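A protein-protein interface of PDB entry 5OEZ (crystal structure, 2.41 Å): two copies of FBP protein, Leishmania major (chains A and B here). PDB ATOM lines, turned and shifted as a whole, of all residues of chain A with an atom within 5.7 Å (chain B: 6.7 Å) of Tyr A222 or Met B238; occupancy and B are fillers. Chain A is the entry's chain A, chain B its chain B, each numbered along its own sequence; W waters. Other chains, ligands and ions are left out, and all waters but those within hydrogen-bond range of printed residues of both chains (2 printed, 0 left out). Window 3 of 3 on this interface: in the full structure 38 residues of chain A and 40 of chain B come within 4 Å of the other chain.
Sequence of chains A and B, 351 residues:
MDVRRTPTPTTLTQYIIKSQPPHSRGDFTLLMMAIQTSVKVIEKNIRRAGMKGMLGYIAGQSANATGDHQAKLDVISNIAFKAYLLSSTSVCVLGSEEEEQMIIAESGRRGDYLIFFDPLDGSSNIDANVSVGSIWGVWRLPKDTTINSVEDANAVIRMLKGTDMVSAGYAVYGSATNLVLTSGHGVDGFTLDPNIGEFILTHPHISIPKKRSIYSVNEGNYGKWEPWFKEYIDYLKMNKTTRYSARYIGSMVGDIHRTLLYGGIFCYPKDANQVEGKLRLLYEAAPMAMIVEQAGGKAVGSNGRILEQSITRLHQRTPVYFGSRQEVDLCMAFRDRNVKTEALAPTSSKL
The side-chain amino group of Lys B237 is in salt-bridge range of the side-chain carboxylate of Glu A219, at 2.7 Å.
OD1 of Asp A234 lies within hydrogen-bond range of OH of Tyr A222 (3.2 Å). The backbone NH (N) of Gly A220 lies within hydrogen-bond range of the side-chain amide oxygen (OD1) of Asn A218 (2.9 Å). NH2 of Arg B243 is in hydrogen-bond range of O of Lys B237 (3.4 Å). The backbone carbonyl oxygen (O) of Asn B239 is in hydrogen-bond range of the guanidinium group (NH2) of Arg B243 (2.8 Å).
OH of Tyr B215 touches C of Glu A219, 3.7 Å away. OH of Tyr B215 touches N of Gly A220 (3.7 Å). CB of Tyr A222 touches CD of Lys B237, at 3.7 Å. Tyr A222 touches Met B238. CD of Arg B243 touches NZ of Lys A224, 3.4 Å away.
Of the printed residues of chain B, Lys A224 touches Arg B243. Of the printed residues of chain B, Glu A219 touches Tyr B215 and Lys B237. Of the printed residues of chain A, Lys B237 touches Glu A219 and Tyr A222. Printed residues of chain B within 4 Å of Gly A220: Tyr B215 (3.7 Å). Of the printed residues of chain A, Arg B243 touches Lys A224 (3.4 Å). Asn B239 touches none of the printed residues of chain A. The nearest residue of chain B that does not touch Tyr A222 is Tyr B215 (6.6 Å). The nearest residue of chain A that does not touch Met B238 is Gly A223 (4.6 Å). The nearest printed residue of chain B that does not touch Lys A224 is Lys B237 (6.2 Å).
Printed residues of chain B that touch a printed residue of chain A: Tyr B215, Lys B237, Met B238 and Arg B243. Among the printed residues, Asp or Glu carboxylates within 4 Å of a Lys or Arg side-chain nitrogen of the other chain: Glu A219 with Lys B237.
Positions printed for both chains: 233 and 234. Of the 6 pairs that touch across the chains among the printed residues, none has its exchanged pair printed and touching as well.
Water W2 lies within hydrogen-bond range of the backbone carbonyl oxygen (O) of Gly A220 (2.7 Å), the backbone NH (N) of Gly A223 (2.8 Å), the backbone carbonyl oxygen (O) of Lys B237 (2.9 Å) and the backbone NH (N) of Tyr A222 (3.1 Å). Water W1 bridges the backbone carbonyl oxygen of Gly A220 (2.8 Å) and the backbone carbonyl oxygen of Leu B236 (2.8 Å).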
ATOM      1  N   ASN A 218      19.614 -12.130  22.155  1.00  0.00           N
ATOM      2  CA  ASN A 218      19.149 -11.011  22.990  1.00  0.00           C
ATOM      3  C   ASN A 218      17.934 -10.339  22.387  1.00  0.00           C
ATOM      4  O   ASN A 218      18.081  -9.474  21.529  1.00  0.00           O
ATOM      5  CB  ASN A 218      20.263  -9.971  23.173  1.00  0.00           C
ATOM      6  CG  ASN A 218      19.873  -8.834  24.115  1.00  0.00           C
ATOM      7  OD1 ASN A 218      18.725  -8.713  24.585  1.00  0.00           O
ATOM      8  ND2 ASN A 218      20.830  -7.960  24.363  1.00  0.00           N
ATOM      9  N   GLU A 219      16.735 -10.702  22.876  1.00  0.00           N
ATOM     10  CA  GLU A 219      15.472 -10.216  22.289  1.00  0.00           C
ATOM     11  C   GLU A 219      15.226  -8.782  22.657  1.00  0.00           C
ATOM     12  O   GLU A 219      14.260  -8.183  22.172  1.00  0.00           O
ATOM     13  CB  GLU A 219      14.268 -11.113  22.653  1.00  0.00           C
ATOM     14  CG  GLU A 219      14.313 -12.506  22.009  1.00  0.00           C
ATOM     15  CD  GLU A 219      12.962 -13.231  21.952  1.00  0.00           C
ATOM     16  OE1 GLU A 219      11.960 -12.620  21.479  1.00  0.00           O
ATOM     17  OE2 GLU A 219      12.887 -14.425  22.364  1.00  0.00           O
ATOM     18  N   GLY A 220      16.054  -8.220  23.541  1.00  0.00           N
ATOM     19  CA  GLY A 220      16.004  -6.779  23.821  1.00  0.00           C
ATOM     20  C   GLY A 220      16.281  -5.913  22.609  1.00  0.00           C
ATOM     21  O   GLY A 220      15.704  -4.843  22.488  1.00  0.00           O
ATOM     22  N   ASN A 221      17.065  -6.439  21.669  1.00  0.00           N
ATOM     23  CA  ASN A 221      17.348  -5.776  20.381  1.00  0.00           C
ATOM     24  C   ASN A 221      16.334  -6.039  19.245  1.00  0.00           C
ATOM     25  O   ASN A 221      16.586  -5.648  18.104  1.00  0.00           O
ATOM     26  CB  ASN A 221      18.734  -6.211  19.902  1.00  0.00           C
ATOM     27  CG  ASN A 221      19.840  -5.769  20.853  1.00  0.00           C
ATOM     28  OD1 ASN A 221      19.752  -4.704  21.447  1.00  0.00           O
ATOM     29  ND2 ASN A 221      20.868  -6.601  21.015  1.00  0.00           N
ATOM     30  N   TYR A 222      15.167  -6.602  19.574  1.00  0.00           N
ATOM     31  CA  TYR A 222      14.106  -6.970  18.595  1.00  0.00           C
ATOM     32  C   TYR A 222      13.806  -5.912  17.552  1.00  0.00           C
ATOM     33  O   TYR A 222      13.840  -6.182  16.360  1.00  0.00           O
ATOM     34  CB  TYR A 222      12.785  -7.290  19.312  1.00  0.00           C
ATOM     35  CG  TYR A 222      11.712  -7.834  18.410  1.00  0.00           C
ATOM     36  CD1 TYR A 222      11.677  -9.171  18.078  1.00  0.00           C
ATOM     37  CD2 TYR A 222      10.746  -7.007  17.881  1.00  0.00           C
ATOM     38  CE1 TYR A 222      10.683  -9.680  17.264  1.00  0.00           C
ATOM     39  CE2 TYR A 222       9.762  -7.499  17.048  1.00  0.00           C
ATOM     40  CZ  TYR A 222       9.745  -8.850  16.750  1.00  0.00           C
ATOM     41  OH  TYR A 222       8.783  -9.354  15.899  1.00  0.00           O
ATOM     42  N   GLY A 223      13.553  -4.698  18.009  1.00  0.00           N
ATOM     43  CA  GLY A 223      13.199  -3.601  17.119  1.00  0.00           C
ATOM     44  C   GLY A 223      14.256  -3.160  16.123  1.00  0.00           C
ATOM     45  O   GLY A 223      13.956  -2.421  15.199  1.00  0.00           O
ATOM     46  N   LYS A 224      15.504  -3.551  16.349  1.00  0.00           N
ATOM     47  CA  LYS A 224      16.596  -3.185  15.472  1.00  0.00           C
ATOM     48  C   LYS A 224      16.896  -4.252  14.420  1.00  0.00           C
ATOM     49  O   LYS A 224      17.743  -4.043  13.576  1.00  0.00           O
ATOM     50  CB  LYS A 224      17.847  -2.968  16.317  1.00  0.00           C
ATOM     51  CG  LYS A 224      17.787  -1.797  17.272  1.00  0.00           C
ATOM     52  CD  LYS A 224      18.610  -2.170  18.478  1.00  0.00           C
ATOM     53  CE  LYS A 224      19.599  -1.045  18.878  1.00  0.00           C
ATOM     54  NZ  LYS A 224      19.182  -0.200  20.040  1.00  0.00           N
ATOM     55  N   TRP A 225      16.278  -5.419  14.530  1.00  0.00           N
ATOM     56  CA  TRP A 225      16.595  -6.543  13.655  1.00  0.00           C
ATOM     57  C   TRP A 225      15.964  -6.413  12.278  1.00  0.00           C
ATOM     58  O   TRP A 225      15.014  -5.659  12.090  1.00  0.00           O
ATOM     59  CB  TRP A 225      16.084  -7.843  14.241  1.00  0.00           C
ATOM     60  CG  TRP A 225      16.760  -8.303  15.465  1.00  0.00           C
ATOM     61  CD1 TRP A 225      18.008  -7.977  15.910  1.00  0.00           C
ATOM     62  CD2 TRP A 225      16.226  -9.238  16.405  1.00  0.00           C
ATOM     63  NE1 TRP A 225      18.273  -8.648  17.070  1.00  0.00           N
ATOM     64  CE2 TRP A 225      17.190  -9.423  17.403  1.00  0.00           C
ATOM     65  CE3 TRP A 225      15.004  -9.922  16.505  1.00  0.00           C
ATOM     66  CZ2 TRP A 225      16.970 -10.265  18.503  1.00  0.00           C
ATOM     67  CZ3 TRP A 225      14.796 -10.770  17.574  1.00  0.00           C
ATOM     68  CH2 TRP A 225      15.769 -10.933  18.560  1.00  0.00           C
ATOM     69  N   LYS A 230      13.139 -11.242  12.535  1.00  0.00           N
ATOM     70  CA  LYS A 230      11.956 -11.110  13.398  1.00  0.00           C
ATOM     71  C   LYS A 230      10.949 -12.222  13.092  1.00  0.00           C
ATOM     72  O   LYS A 230      10.406 -12.839  14.016  1.00  0.00           O
ATOM     73  CB  LYS A 230      11.260  -9.779  13.206  1.00  0.00           C
ATOM     74  CG  LYS A 230      12.058  -8.579  13.655  1.00  0.00           C
ATOM     75  CD  LYS A 230      11.199  -7.337  13.468  1.00  0.00           C
ATOM     76  CE  LYS A 230      11.961  -6.090  13.826  1.00  0.00           C
ATOM     77  NZ  LYS A 230      11.222  -4.910  13.347  1.00  0.00           N
ATOM     78  N   GLU A 231      10.746 -12.498  11.805  1.00  0.00           N
ATOM     79  CA  GLU A 231       9.822 -13.559  11.405  1.00  0.00           C
ATOM     80  C   GLU A 231      10.273 -14.911  11.920  1.00  0.00           C
ATOM     81  O   GLU A 231       9.443 -15.711  12.373  1.00  0.00           O
ATOM     82  CB  GLU A 231       9.620 -13.582   9.890  1.00  0.00           C
ATOM     83  CG  GLU A 231       8.843 -12.368   9.412  1.00  0.00           C
ATOM     84  CD  GLU A 231       8.417 -12.373   7.959  1.00  0.00           C
ATOM     85  OE1 GLU A 231       8.012 -13.432   7.479  1.00  0.00           O
ATOM     86  OE2 GLU A 231       8.389 -11.293   7.332  1.00  0.00           O
ATOM     87  N   ILE A 233      12.178 -15.527  14.569  1.00  0.00           N
ATOM     88  CA  ILE A 233      11.994 -15.567  16.017  1.00  0.00           C
ATOM     89  C   ILE A 233      10.507 -15.724  16.367  1.00  0.00           C
ATOM     90  O   ILE A 233      10.180 -16.547  17.223  1.00  0.00           O
ATOM     91  CB  ILE A 233      12.661 -14.364  16.729  1.00  0.00           C
ATOM     92  CG1 ILE A 233      14.197 -14.437  16.570  1.00  0.00           C
ATOM     93  CG2 ILE A 233      12.309 -14.326  18.208  1.00  0.00           C
ATOM     94  CD1 ILE A 233      14.889 -15.634  17.214  1.00  0.00           C
ATOM     95  N   ASP A 234       9.628 -15.001  15.674  1.00  0.00           N
ATOM     96  CA  ASP A 234       8.190 -15.143  15.888  1.00  0.00           C
ATOM     97  C   ASP A 234       7.718 -16.586  15.618  1.00  0.00           C
ATOM     98  O   ASP A 234       6.883 -17.117  16.346  1.00  0.00           O
ATOM     99  CB  ASP A 234       7.399 -14.147  15.035  1.00  0.00           C
ATOM    100  CG  ASP A 234       7.577 -12.692  15.483  1.00  0.00           C
ATOM    101  OD1 ASP A 234       8.291 -12.430  16.492  1.00  0.00           O
ATOM    102  OD2 ASP A 234       7.002 -11.803  14.807  1.00  0.00           O
ATOM    103  N   TYR B 215      15.510  -7.184  31.696  1.00  0.00           N
ATOM    104  CA  TYR B 215      14.414  -8.101  32.006  1.00  0.00           C
ATOM    105  C   TYR B 215      14.854  -9.533  31.760  1.00  0.00           C
ATOM    106  O   TYR B 215      15.641  -9.823  30.852  1.00  0.00           O
ATOM    107  CB  TYR B 215      13.138  -7.750  31.225  1.00  0.00           C
ATOM    108  CG  TYR B 215      13.150  -8.090  29.756  1.00  0.00           C
ATOM    109  CD1 TYR B 215      13.752  -7.247  28.835  1.00  0.00           C
ATOM    110  CD2 TYR B 215      12.569  -9.276  29.285  1.00  0.00           C
ATOM    111  CE1 TYR B 215      13.759  -7.546  27.480  1.00  0.00           C
ATOM    112  CE2 TYR B 215      12.587  -9.593  27.935  1.00  0.00           C
ATOM    113  CZ  TYR B 215      13.178  -8.713  27.032  1.00  0.00           C
ATOM    114  OH  TYR B 215      13.193  -9.007  25.686  1.00  0.00           O
ATOM    115  N   ILE B 233       5.860  -7.287  27.651  1.00  0.00           N
ATOM    116  CA  ILE B 233       7.113  -7.709  27.018  1.00  0.00           C
ATOM    117  C   ILE B 233       7.308  -7.021  25.676  1.00  0.00           C
ATOM    118  O   ILE B 233       8.400  -6.516  25.400  1.00  0.00           O
ATOM    119  CB  ILE B 233       7.224  -9.243  26.914  1.00  0.00           C
ATOM    120  CG1 ILE B 233       7.303  -9.857  28.325  1.00  0.00           C
ATOM    121  CG2 ILE B 233       8.433  -9.670  26.090  1.00  0.00           C
ATOM    122  CD1 ILE B 233       8.526  -9.478  29.148  1.00  0.00           C
ATOM    123  N   ASP B 234       6.247  -6.926  24.873  1.00  0.00           N
ATOM    124  CA  ASP B 234       6.331  -6.194  23.592  1.00  0.00           C
ATOM    125  C   ASP B 234       6.739  -4.735  23.807  1.00  0.00           C
ATOM    126  O   ASP B 234       7.507  -4.172  23.018  1.00  0.00           O
ATOM    127  CB  ASP B 234       5.011  -6.280  22.798  1.00  0.00           C
ATOM    128  CG  ASP B 234       4.715  -7.695  22.250  1.00  0.00           C
ATOM    129  OD1 ASP B 234       5.517  -8.630  22.451  1.00  0.00           O
ATOM    130  OD2 ASP B 234       3.614  -7.883  21.683  1.00  0.00           O
ATOM    131  N   TYR B 235       6.212  -4.122  24.865  1.00  0.00           N
ATOM    132  CA  TYR B 235       6.541  -2.743  25.195  1.00  0.00           C
ATOM    133  C   TYR B 235       8.029  -2.582  25.522  1.00  0.00           C
ATOM    134  O   TYR B 235       8.670  -1.692  24.990  1.00  0.00           O
ATOM    135  CB  TYR B 235       5.681  -2.236  26.371  1.00  0.00           C
ATOM    136  CG  TYR B 235       6.010  -0.828  26.798  1.00  0.00           C
ATOM    137  CD1 TYR B 235       5.484   0.259  26.109  1.00  0.00           C
ATOM    138  CD2 TYR B 235       6.865  -0.584  27.876  1.00  0.00           C
ATOM    139  CE1 TYR B 235       5.790   1.553  26.488  1.00  0.00           C
ATOM    140  CE2 TYR B 235       7.174   0.706  28.263  1.00  0.00           C
ATOM    141  CZ  TYR B 235       6.636   1.767  27.567  1.00  0.00           C
ATOM    142  OH  TYR B 235       6.939   3.050  27.932  1.00  0.00           O
ATOM    143  N   LEU B 236       8.560  -3.436  26.390  1.00  0.00           N
ATOM    144  CA  LEU B 236       9.993  -3.431  26.697  1.00  0.00           C
ATOM    145  C   LEU B 236      10.871  -3.463  25.440  1.00  0.00           C
ATOM    146  O   LEU B 236      11.850  -2.738  25.350  1.00  0.00           O
ATOM    147  CB  LEU B 236      10.371  -4.598  27.597  1.00  0.00           C
ATOM    148  CG  LEU B 236       9.745  -4.732  28.989  1.00  0.00           C
ATOM    149  CD1 LEU B 236      10.479  -5.820  29.746  1.00  0.00           C
ATOM    150  CD2 LEU B 236       9.770  -3.441  29.782  1.00  0.00           C
ATOM    151  N   LYS B 237      10.484  -4.253  24.451  1.00  0.00           N
ATOM    152  CA  LYS B 237      11.237  -4.342  23.202  1.00  0.00           C
ATOM    153  C   LYS B 237      11.024  -3.217  22.193  1.00  0.00           C
ATOM    154  O   LYS B 237      11.895  -2.948  21.372  1.00  0.00           O
ATOM    155  CB  LYS B 237      10.838  -5.598  22.486  1.00  0.00           C
ATOM    156  CG  LYS B 237      11.057  -6.866  23.256  1.00  0.00           C
ATOM    157  CD  LYS B 237      10.659  -7.977  22.317  1.00  0.00           C
ATOM    158  CE  LYS B 237      10.711  -9.305  23.001  1.00  0.00           C
ATOM    159  NZ  LYS B 237      10.633 -10.344  21.944  1.00  0.00           N
ATOM    160  N   MET B 238       9.833  -2.620  22.164  1.00  0.00           N
ATOM    161  CA  MET B 238       9.479  -1.723  21.053  1.00  0.00           C
ATOM    162  C   MET B 238       9.090  -0.306  21.427  1.00  0.00           C
ATOM    163  O   MET B 238       8.829   0.481  20.539  1.00  0.00           O
ATOM    164  CB  MET B 238       8.430  -2.405  20.183  1.00  0.00           C
ATOM    165  CG  MET B 238       9.152  -3.392  19.266  1.00  0.00           C
ATOM    166  SD  MET B 238       8.225  -4.707  18.508  1.00  0.00           S
ATOM    167  CE  MET B 238       7.416  -5.523  19.900  1.00  0.00           C
ATOM    168  N   ASN B 239       9.086   0.043  22.711  1.00  0.00           N
ATOM    169  CA  ASN B 239       8.845   1.437  23.113  1.00  0.00           C
ATOM    170  C   ASN B 239       9.955   2.350  22.581  1.00  0.00           C
ATOM    171  O   ASN B 239      11.092   1.908  22.420  1.00  0.00           O
ATOM    172  CB  ASN B 239       8.694   1.567  24.645  1.00  0.00           C
ATOM    173  CG  ASN B 239      10.019   1.556  25.380  1.00  0.00           C
ATOM    174  OD1 ASN B 239      10.562   2.614  25.684  1.00  0.00           O
ATOM    175  ND2 ASN B 239      10.557   0.375  25.652  1.00  0.00           N
ATOM    176  N   LYS B 240       9.618   3.613  22.338  1.00  0.00           N
ATOM    177  CA  LYS B 240      10.527   4.579  21.700  1.00  0.00           C
ATOM    178  C   LYS B 240      11.499   5.255  22.696  1.00  0.00           C
ATOM    179  O   LYS B 240      12.484   5.872  22.289  1.00  0.00           O
ATOM    180  CB  LYS B 240       9.709   5.623  20.899  1.00  0.00           C
ATOM    181  CG  LYS B 240       8.905   6.638  21.735  1.00  0.00           C
ATOM    182  CD  LYS B 240       8.231   7.779  20.916  1.00  0.00           C
ATOM    183  CE  LYS B 240       7.274   7.312  19.834  1.00  0.00           C
ATOM    184  NZ  LYS B 240       6.196   6.428  20.328  1.00  0.00           N
ATOM    185  N   THR B 241      11.249   5.087  23.990  1.00  0.00           N
ATOM    186  CA  THR B 241      11.900   5.866  25.040  1.00  0.00           C
ATOM    187  C   THR B 241      13.103   5.164  25.695  1.00  0.00           C
ATOM    188  O   THR B 241      14.151   5.788  25.892  1.00  0.00           O
ATOM    189  CB  THR B 241      10.821   6.236  26.113  1.00  0.00           C
ATOM    190  OG1 THR B 241       9.838   7.089  25.519  1.00  0.00           O
ATOM    191  CG2 THR B 241      11.395   6.937  27.344  1.00  0.00           C
ATOM    192  N   THR B 242      12.967   3.880  26.022  1.00  0.00           N
ATOM    193  CA  THR B 242      13.938   3.162  26.869  1.00  0.00           C
ATOM    194  C   THR B 242      14.331   1.808  26.266  1.00  0.00           C
ATOM    195  O   THR B 242      13.474   0.948  26.076  1.00  0.00           O
ATOM    196  CB  THR B 242      13.344   2.939  28.281  1.00  0.00           C
ATOM    197  OG1 THR B 242      12.765   4.153  28.753  1.00  0.00           O
ATOM    198  CG2 THR B 242      14.387   2.461  29.309  1.00  0.00           C
ATOM    199  N   ARG B 243      15.624   1.612  26.003  1.00  0.00           N
ATOM    200  CA  ARG B 243      16.136   0.340  25.487  1.00  0.00           C
ATOM    201  C   ARG B 243      16.382  -0.632  26.629  1.00  0.00           C
ATOM    202  O   ARG B 243      16.974  -0.249  27.629  1.00  0.00           O
ATOM    203  CB  ARG B 243      17.423   0.542  24.682  1.00  0.00           C
ATOM    204  CG  ARG B 243      17.246   1.399  23.430  1.00  0.00           C
ATOM    205  CD  ARG B 243      16.734   0.615  22.221  1.00  0.00           C
ATOM    206  NE  ARG B 243      15.415   0.015  22.441  1.00  0.00           N
ATOM    207  CZ  ARG B 243      14.247   0.666  22.431  1.00  0.00           C
ATOM    208  NH1 ARG B 243      14.183   1.980  22.207  1.00  0.00           N
ATOM    209  NH2 ARG B 243      13.118  -0.013  22.658  1.00  0.00           N
HETATM  210  O   HOH W   1      14.368  -3.003  24.102  1.00  0.00           O
HETATM  211  O   HOH W   2      14.527  -3.659  20.380  1.00  0.00           O
